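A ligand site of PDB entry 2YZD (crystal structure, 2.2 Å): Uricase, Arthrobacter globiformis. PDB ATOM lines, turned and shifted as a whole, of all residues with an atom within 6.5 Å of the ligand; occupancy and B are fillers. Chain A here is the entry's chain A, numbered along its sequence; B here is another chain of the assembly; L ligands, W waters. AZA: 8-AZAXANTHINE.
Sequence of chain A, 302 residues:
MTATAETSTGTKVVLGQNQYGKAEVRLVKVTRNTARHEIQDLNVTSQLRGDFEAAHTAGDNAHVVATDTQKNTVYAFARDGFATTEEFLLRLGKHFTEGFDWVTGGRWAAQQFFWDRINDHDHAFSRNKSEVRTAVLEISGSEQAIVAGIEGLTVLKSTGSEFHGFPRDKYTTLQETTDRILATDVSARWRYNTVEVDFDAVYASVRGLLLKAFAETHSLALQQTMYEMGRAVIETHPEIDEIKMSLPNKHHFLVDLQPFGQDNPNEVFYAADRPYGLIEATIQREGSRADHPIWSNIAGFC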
ATOM      1  N   GLU A 162     -12.700  -8.830  21.649  1.00  0.00           N
ATOM      2  CA  GLU A 162     -13.307  -8.202  20.480  1.00  0.00           C
ATOM      3  C   GLU A 162     -14.344  -9.105  19.851  1.00  0.00           C
ATOM      4  O   GLU A 162     -14.428 -10.296  20.169  1.00  0.00           O
ATOM      5  CB  GLU A 162     -12.246  -7.766  19.461  1.00  0.00           C
ATOM      6  CG  GLU A 162     -11.116  -8.725  19.194  1.00  0.00           C
ATOM      7  CD  GLU A 162     -10.018  -8.090  18.329  1.00  0.00           C
ATOM      8  OE1 GLU A 162     -10.323  -7.640  17.203  1.00  0.00           O
ATOM      9  OE2 GLU A 162      -8.857  -8.044  18.793  1.00  0.00           O
ATOM     10  N   PHE A 163     -15.174  -8.537  18.988  1.00  0.00           N
ATOM     11  CA  PHE A 163     -16.211  -9.301  18.324  1.00  0.00           C
ATOM     12  C   PHE A 163     -16.573  -8.667  16.995  1.00  0.00           C
ATOM     13  O   PHE A 163     -17.252  -7.638  16.930  1.00  0.00           O
ATOM     14  CB  PHE A 163     -17.468  -9.394  19.198  1.00  0.00           C
ATOM     15  CG  PHE A 163     -18.530 -10.292  18.631  1.00  0.00           C
ATOM     16  CD1 PHE A 163     -18.297 -11.652  18.482  1.00  0.00           C
ATOM     17  CD2 PHE A 163     -19.751  -9.771  18.215  1.00  0.00           C
ATOM     18  CE1 PHE A 163     -19.253 -12.489  17.916  1.00  0.00           C
ATOM     19  CE2 PHE A 163     -20.717 -10.604  17.649  1.00  0.00           C
ATOM     20  CZ  PHE A 163     -20.472 -11.961  17.507  1.00  0.00           C
ATOM     21  N   PHE A 166     -18.947 -11.039  12.040  1.00  0.00           N
ATOM     22  CA  PHE A 166     -20.224 -11.749  12.072  1.00  0.00           C
ATOM     23  C   PHE A 166     -21.091 -11.306  10.894  1.00  0.00           C
ATOM     24  O   PHE A 166     -20.882 -10.234  10.340  1.00  0.00           O
ATOM     25  CB  PHE A 166     -20.963 -11.515  13.397  1.00  0.00           C
ATOM     26  CG  PHE A 166     -21.091 -10.065  13.781  1.00  0.00           C
ATOM     27  CD1 PHE A 166     -20.118  -9.447  14.570  1.00  0.00           C
ATOM     28  CD2 PHE A 166     -22.188  -9.297  13.364  1.00  0.00           C
ATOM     29  CE1 PHE A 166     -20.230  -8.106  14.938  1.00  0.00           C
ATOM     30  CE2 PHE A 166     -22.309  -7.952  13.732  1.00  0.00           C
ATOM     31  CZ  PHE A 166     -21.324  -7.355  14.523  1.00  0.00           C
ATOM     32  N   LEU A 174     -25.827  -4.488  15.392  1.00  0.00           N
ATOM     33  CA  LEU A 174     -24.661  -4.566  16.252  1.00  0.00           C
ATOM     34  C   LEU A 174     -23.453  -4.168  15.418  1.00  0.00           C
ATOM     35  O   LEU A 174     -23.306  -4.629  14.285  1.00  0.00           O
ATOM     36  CB  LEU A 174     -24.458  -5.992  16.777  1.00  0.00           C
ATOM     37  CG  LEU A 174     -23.212  -6.230  17.648  1.00  0.00           C
ATOM     38  CD1 LEU A 174     -23.391  -5.545  18.996  1.00  0.00           C
ATOM     39  CD2 LEU A 174     -22.986  -7.725  17.824  1.00  0.00           C
ATOM     40  N   ARG A 180     -13.917  -4.295  23.847  1.00  0.00           N
ATOM     41  CA  ARG A 180     -15.136  -4.245  24.637  1.00  0.00           C
ATOM     42  C   ARG A 180     -14.896  -5.002  25.946  1.00  0.00           C
ATOM     43  O   ARG A 180     -13.865  -5.661  26.106  1.00  0.00           O
ATOM     44  CB  ARG A 180     -16.282  -4.923  23.872  1.00  0.00           C
ATOM     45  CG  ARG A 180     -16.057  -6.419  23.715  1.00  0.00           C
ATOM     46  CD  ARG A 180     -17.219  -7.186  23.088  1.00  0.00           C
ATOM     47  NE  ARG A 180     -16.935  -8.627  23.100  1.00  0.00           N
ATOM     48  CZ  ARG A 180     -17.784  -9.585  22.744  1.00  0.00           C
ATOM     49  NH1 ARG A 180     -19.026  -9.272  22.337  1.00  0.00           N
ATOM     50  NH2 ARG A 180     -17.401 -10.852  22.808  1.00  0.00           N
ATOM     51  N   LEU A 182     -15.814  -8.032  28.460  1.00  0.00           N
ATOM     52  CA  LEU A 182     -16.344  -9.388  28.356  1.00  0.00           C
ATOM     53  C   LEU A 182     -16.598  -9.835  29.785  1.00  0.00           C
ATOM     54  O   LEU A 182     -15.647 -10.033  30.557  1.00  0.00           O
ATOM     55  CB  LEU A 182     -15.339 -10.317  27.686  1.00  0.00           C
ATOM     56  CG  LEU A 182     -15.831 -11.762  27.539  1.00  0.00           C
ATOM     57  CD1 LEU A 182     -17.083 -11.779  26.658  1.00  0.00           C
ATOM     58  CD2 LEU A 182     -14.727 -12.635  26.933  1.00  0.00           C
ATOM     59  N   SER A 219      -9.829 -12.798  23.523  1.00  0.00           N
ATOM     60  CA  SER A 219     -11.110 -13.212  22.973  1.00  0.00           C
ATOM     61  C   SER A 219     -11.604 -12.546  21.708  1.00  0.00           C
ATOM     62  O   SER A 219     -11.626 -11.316  21.597  1.00  0.00           O
ATOM     63  CB  SER A 219     -12.190 -13.085  24.042  1.00  0.00           C
ATOM     64  OG  SER A 219     -13.398 -13.662  23.595  1.00  0.00           O
ATOM     65  N   LEU A 220     -12.029 -13.384  20.761  1.00  0.00           N
ATOM     66  CA  LEU A 220     -12.580 -12.942  19.477  1.00  0.00           C
ATOM     67  C   LEU A 220     -14.087 -13.242  19.486  1.00  0.00           C
ATOM     68  O   LEU A 220     -14.814 -12.919  18.533  1.00  0.00           O
ATOM     69  CB  LEU A 220     -11.920 -13.680  18.315  1.00  0.00           C
ATOM     70  CG  LEU A 220     -10.440 -13.351  18.069  1.00  0.00           C
ATOM     71  CD1 LEU A 220      -9.931 -14.137  16.868  1.00  0.00           C
ATOM     72  CD2 LEU A 220     -10.280 -11.866  17.825  1.00  0.00           C
ATOM     73  N   ALA A 221     -14.533 -13.868  20.568  1.00  0.00           N
ATOM     74  CA  ALA A 221     -15.927 -14.229  20.797  1.00  0.00           C
ATOM     75  C   ALA A 221     -16.012 -15.048  22.074  1.00  0.00           C
ATOM     76  O   ALA A 221     -15.062 -15.765  22.411  1.00  0.00           O
ATOM     77  CB  ALA A 221     -16.466 -15.036  19.618  1.00  0.00           C
ATOM     78  N   LEU A 222     -17.125 -14.947  22.789  1.00  0.00           N
ATOM     79  CA  LEU A 222     -17.278 -15.704  24.031  1.00  0.00           C
ATOM     80  C   LEU A 222     -17.122 -17.181  23.721  1.00  0.00           C
ATOM     81  O   LEU A 222     -16.612 -17.945  24.538  1.00  0.00           O
ATOM     82  CB  LEU A 222     -18.655 -15.468  24.671  1.00  0.00           C
ATOM     83  CG  LEU A 222     -18.662 -15.341  26.195  1.00  0.00           C
ATOM     84  CD1 LEU A 222     -20.083 -15.408  26.728  1.00  0.00           C
ATOM     85  CD2 LEU A 222     -17.811 -16.425  26.816  1.00  0.00           C
ATOM     86  N   GLN A 223     -17.595 -17.582  22.538  1.00  0.00           N
ATOM     87  CA  GLN A 223     -17.510 -18.968  22.079  1.00  0.00           C
ATOM     88  C   GLN A 223     -16.063 -19.467  22.078  1.00  0.00           C
ATOM     89  O   GLN A 223     -15.788 -20.588  22.464  1.00  0.00           O
ATOM     90  CB  GLN A 223     -18.078 -19.107  20.659  1.00  0.00           C
ATOM     91  CG  GLN A 223     -19.606 -19.113  20.547  1.00  0.00           C
ATOM     92  CD  GLN A 223     -20.211 -17.714  20.424  1.00  0.00           C
ATOM     93  OE1 GLN A 223     -19.623 -16.733  20.875  1.00  0.00           O
ATOM     94  NE2 GLN A 223     -21.388 -17.624  19.818  1.00  0.00           N
ATOM     95  N   ASN A 249     -23.351 -13.757  28.488  1.00  0.00           N
ATOM     96  CA  ASN A 249     -22.569 -12.596  28.073  1.00  0.00           C
ATOM     97  C   ASN A 249     -23.265 -11.404  28.743  1.00  0.00           C
ATOM     98  O   ASN A 249     -24.265 -10.894  28.223  1.00  0.00           O
ATOM     99  CB  ASN A 249     -22.598 -12.441  26.548  1.00  0.00           C
ATOM    100  CG  ASN A 249     -21.547 -11.455  26.025  1.00  0.00           C
ATOM    101  OD1 ASN A 249     -20.754 -10.894  26.796  1.00  0.00           O
ATOM    102  ND2 ASN A 249     -21.532 -11.244  24.719  1.00  0.00           N
ATOM    103  N   HIS A 251     -23.820  -7.990  29.253  1.00  0.00           N
ATOM    104  CA  HIS A 251     -23.589  -6.746  28.563  1.00  0.00           C
ATOM    105  C   HIS A 251     -23.314  -5.508  29.392  1.00  0.00           C
ATOM    106  O   HIS A 251     -24.072  -5.138  30.285  1.00  0.00           O
ATOM    107  CB  HIS A 251     -24.740  -6.509  27.583  1.00  0.00           C
ATOM    108  CG  HIS A 251     -24.947  -7.642  26.624  1.00  0.00           C
ATOM    109  ND1 HIS A 251     -26.192  -8.158  26.336  1.00  0.00           N
ATOM    110  CD2 HIS A 251     -24.057  -8.394  25.926  1.00  0.00           C
ATOM    111  CE1 HIS A 251     -26.061  -9.187  25.506  1.00  0.00           C
ATOM    112  NE2 HIS A 251     -24.781  -9.343  25.248  1.00  0.00           N
ATOM    113  N   ILE A 279     -24.113 -18.316  25.847  1.00  0.00           N
ATOM    114  CA  ILE A 279     -23.245 -19.156  25.025  1.00  0.00           C
ATOM    115  C   ILE A 279     -22.895 -20.417  25.810  1.00  0.00           C
ATOM    116  O   ILE A 279     -22.216 -20.357  26.842  1.00  0.00           O
ATOM    117  CB  ILE A 279     -21.957 -18.376  24.643  1.00  0.00           C
ATOM    118  CG1 ILE A 279     -22.281 -17.283  23.633  1.00  0.00           C
ATOM    119  CG2 ILE A 279     -20.919 -19.319  24.045  1.00  0.00           C
ATOM    120  CD1 ILE A 279     -23.196 -16.181  24.143  1.00  0.00           C
ATOM    121  N   TYR B  20     -26.201 -21.295  21.189  1.00  0.00           N
ATOM    122  CA  TYR B  20     -26.004 -19.937  21.683  1.00  0.00           C
ATOM    123  C   TYR B  20     -27.120 -19.031  21.181  1.00  0.00           C
ATOM    124  O   TYR B  20     -27.758 -19.335  20.170  1.00  0.00           O
ATOM    125  CB  TYR B  20     -24.661 -19.389  21.187  1.00  0.00           C
ATOM    126  CG  TYR B  20     -24.768 -18.836  19.781  1.00  0.00           C
ATOM    127  CD1 TYR B  20     -24.881 -19.690  18.684  1.00  0.00           C
ATOM    128  CD2 TYR B  20     -24.871 -17.463  19.559  1.00  0.00           C
ATOM    129  CE1 TYR B  20     -25.111 -19.194  17.396  1.00  0.00           C
ATOM    130  CE2 TYR B  20     -25.107 -16.955  18.292  1.00  0.00           C
ATOM    131  CZ  TYR B  20     -25.230 -17.827  17.217  1.00  0.00           C
ATOM    132  OH  TYR B  20     -25.494 -17.330  15.956  1.00  0.00           O
ATOM    133  N   GLY B  21     -27.330 -17.907  21.860  1.00  0.00           N
ATOM    134  CA  GLY B  21     -28.357 -16.961  21.459  1.00  0.00           C
ATOM    135  C   GLY B  21     -28.660 -15.893  22.506  1.00  0.00           C
ATOM    136  O   GLY B  21     -27.838 -15.616  23.370  1.00  0.00           O
ATOM    137  N   LYS B  22     -29.830 -15.284  22.421  1.00  0.00           N
ATOM    138  CA  LYS B  22     -30.196 -14.267  23.397  1.00  0.00           C
ATOM    139  C   LYS B  22     -31.250 -14.795  24.343  1.00  0.00           C
ATOM    140  O   LYS B  22     -32.315 -15.250  23.925  1.00  0.00           O
ATOM    141  CB  LYS B  22     -30.726 -12.998  22.717  1.00  0.00           C
ATOM    142  CG  LYS B  22     -30.909 -11.824  23.686  1.00  0.00           C
ATOM    143  CD  LYS B  22     -29.558 -11.205  24.094  1.00  0.00           C
ATOM    144  CE  LYS B  22     -28.959 -10.402  22.938  1.00  0.00           C
ATOM    145  NZ  LYS B  22     -27.571  -9.914  23.198  1.00  0.00           N
ATOM    146  N   ASN B  61     -16.089 -15.802  13.230  1.00  0.00           N
ATOM    147  CA  ASN B  61     -17.516 -15.563  13.464  1.00  0.00           C
ATOM    148  C   ASN B  61     -18.436 -15.478  12.252  1.00  0.00           C
ATOM    149  O   ASN B  61     -19.571 -15.004  12.373  1.00  0.00           O
ATOM    150  CB  ASN B  61     -17.687 -14.305  14.330  1.00  0.00           C
ATOM    151  CG  ASN B  61     -16.952 -14.417  15.655  1.00  0.00           C
ATOM    152  OD1 ASN B  61     -17.193 -15.335  16.421  1.00  0.00           O
ATOM    153  ND2 ASN B  61     -16.060 -13.473  15.922  1.00  0.00           N
ATOM    154  N   VAL B  64     -21.785 -16.852  12.989  1.00  0.00           N
ATOM    155  CA  VAL B  64     -22.466 -16.369  14.177  1.00  0.00           C
ATOM    156  C   VAL B  64     -23.483 -15.249  14.009  1.00  0.00           C
ATOM    157  O   VAL B  64     -23.121 -14.075  14.037  1.00  0.00           O
ATOM    158  CB  VAL B  64     -21.434 -15.964  15.270  1.00  0.00           C
ATOM    159  CG1 VAL B  64     -22.149 -15.633  16.577  1.00  0.00           C
ATOM    160  CG2 VAL B  64     -20.416 -17.098  15.496  1.00  0.00           C
ATOM    161  N   VAL B  65     -24.743 -15.614  13.826  1.00  0.00           N
ATOM    162  CA  VAL B  65     -25.813 -14.623  13.733  1.00  0.00           C
ATOM    163  C   VAL B  65     -25.862 -14.051  15.155  1.00  0.00           C
ATOM    164  O   VAL B  65     -26.289 -14.729  16.092  1.00  0.00           O
ATOM    165  CB  VAL B  65     -27.164 -15.302  13.413  1.00  0.00           C
ATOM    166  CG1 VAL B  65     -28.283 -14.263  13.379  1.00  0.00           C
ATOM    167  CG2 VAL B  65     -27.064 -16.035  12.086  1.00  0.00           C
ATOM    168  N   ALA B  66     -25.394 -12.821  15.319  1.00  0.00           N
ATOM    169  CA  ALA B  66     -25.329 -12.164  16.628  1.00  0.00           C
ATOM    170  C   ALA B  66     -26.536 -12.381  17.546  1.00  0.00           C
ATOM    171  O   ALA B  66     -27.675 -12.429  17.076  1.00  0.00           O
ATOM    172  CB  ALA B  66     -25.076 -10.658  16.444  1.00  0.00           C
ATOM    173  N   THR B  67     -26.283 -12.513  18.845  1.00  0.00           N
ATOM    174  CA  THR B  67     -27.374 -12.689  19.794  1.00  0.00           C
ATOM    175  C   THR B  67     -28.200 -11.404  19.724  1.00  0.00           C
ATOM    176  O   THR B  67     -29.424 -11.434  19.852  1.00  0.00           O
ATOM    177  CB  THR B  67     -26.870 -12.901  21.249  1.00  0.00           C
ATOM    178  OG1 THR B  67     -26.252 -11.707  21.740  1.00  0.00           O
ATOM    179  CG2 THR B  67     -25.878 -14.045  21.290  1.00  0.00           C
ATOM    180  N   ASP B  68     -27.513 -10.279  19.499  1.00  0.00           N
ATOM    181  CA  ASP B  68     -28.178  -8.985  19.386  1.00  0.00           C
ATOM    182  C   ASP B  68     -29.171  -9.028  18.227  1.00  0.00           C
ATOM    183  O   ASP B  68     -30.263  -8.466  18.317  1.00  0.00           O
ATOM    184  CB  ASP B  68     -27.163  -7.873  19.118  1.00  0.00           C
ATOM    185  CG  ASP B  68     -27.792  -6.481  19.157  1.00  0.00           C
ATOM    186  OD1 ASP B  68     -28.215  -6.027  20.244  1.00  0.00           O
ATOM    187  OD2 ASP B  68     -27.887  -5.831  18.087  1.00  0.00           O
ATOM    188  N   THR B  69     -28.783  -9.701  17.150  1.00  0.00           N
ATOM    189  CA  THR B  69     -29.642  -9.838  15.973  1.00  0.00           C
ATOM    190  C   THR B  69     -30.873 -10.668  16.310  1.00  0.00           C
ATOM    191  O   THR B  69     -32.000 -10.346  15.908  1.00  0.00           O
ATOM    192  CB  THR B  69     -28.891 -10.501  14.804  1.00  0.00           C
ATOM    193  OG1 THR B  69     -27.845  -9.635  14.344  1.00  0.00           O
ATOM    194  CG2 THR B  69     -29.846 -10.772  13.651  1.00  0.00           C
ATOM    195  N   GLN B  70     -30.665 -11.740  17.052  1.00  0.00           N
ATOM    196  CA  GLN B  70     -31.768 -12.597  17.439  1.00  0.00           C
ATOM    197  C   GLN B  70     -32.761 -11.785  18.279  1.00  0.00           C
ATOM    198  O   GLN B  70     -33.976 -11.929  18.136  1.00  0.00           O
ATOM    199  CB  GLN B  70     -31.228 -13.806  18.201  1.00  0.00           C
ATOM    200  CG  GLN B  70     -30.314 -14.653  17.310  1.00  0.00           C
ATOM    201  CD  GLN B  70     -29.735 -15.859  18.010  1.00  0.00           C
ATOM    202  OE1 GLN B  70     -30.457 -16.677  18.588  1.00  0.00           O
ATOM    203  NE2 GLN B  70     -28.401 -15.987  17.966  1.00  0.00           N
HETATM  204  N1  AZA L   1     -20.799 -14.046  20.856  1.00  0.00           N
HETATM  205  C2  AZA L   1     -20.110 -13.014  21.478  1.00  0.00           C
HETATM  206  O2  AZA L   1     -19.054 -13.204  22.056  1.00  0.00           O
HETATM  207  N3  AZA L   1     -20.650 -11.728  21.428  1.00  0.00           N
HETATM  208  C4  AZA L   1     -21.823 -11.517  20.773  1.00  0.00           C
HETATM  209  C5  AZA L   1     -22.516 -12.533  20.150  1.00  0.00           C
HETATM  210  C6  AZA L   1     -22.018 -13.916  20.168  1.00  0.00           C
HETATM  211  O6  AZA L   1     -22.541 -14.906  19.657  1.00  0.00           O
HETATM  212  N7  AZA L   1     -23.621 -12.015  19.604  1.00  0.00           N
HETATM  213  N8  AZA L   1     -23.546 -10.707  19.918  1.00  0.00           N
HETATM  214  N9  AZA L   1     -22.450 -10.359  20.633  1.00  0.00           N
HETATM  215  O   HOH W   1     -23.891 -12.326  23.470  1.00  0.00           O
HETATM  216  O   HOH W   2     -22.226  -7.875  21.916  1.00  0.00           O
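N of Leu 222 sits at hydrogen-bond distance from O2 of the ligand, at 2.7 Å.
A nitrogen (N7) of the ligand sits at hydrogen-bond distance from the backbone NH (N) of Thr 67 of chain B (2.8 Å).
The side-chain hydroxyl of Thr 67 of chain B sits at hydrogen-bond distance from a nitrogen (N7) of the ligand (3.4 Å).
The side-chain amide oxygen of Gln 223 sits at hydrogen-bond distance from a nitrogen (N1) of the ligand, at 2.9 Å.
The guanidinium group of Arg 180 is in hydrogen-bond range of an oxygen (O2) of the ligand, at 3.0 Å.
A nitrogen (N3) of the ligand sits close to the side-chain amide nitrogen (ND2) of Asn 249, at 3.4 Å.
Phe 163 touches the ligand.
CD2 of Leu 174 touches N8 of the ligand (3.7 Å).
CA of Ala 221 touches O2 of the ligand, 3.5 Å away.
Tyr 20 of chain B touches the ligand (CD2 to O6, 3.5 Å).
Val 64 of chain B touches the ligand (CG1 to O6, 3.2 Å).
CA of Ala 66 of chain B touches N7 of the ligand (3.4 Å).
The side-chain hydroxyl of Thr 67 of chain B is in hydrogen-bond range of the side-chain amino group of Lys 22 of chain B (2.7 Å).
The backbone carbonyl oxygen of Asn 249 is in hydrogen-bond range of a ring nitrogen (NE2) of His 251.
O of Val 65 of chain B sits at hydrogen-bond distance from OH of Tyr 20 of chain B (2.7 Å).
The backbone carbonyl oxygen (O) of Ala 221 sits at hydrogen-bond distance from the side-chain hydroxyl (OG) of Ser 219, at 2.9 Å.
Water W1 bridges ND2 of Asn 249 (2.9 Å) and OG1 of Thr 67 of chain B (3.0 Å).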
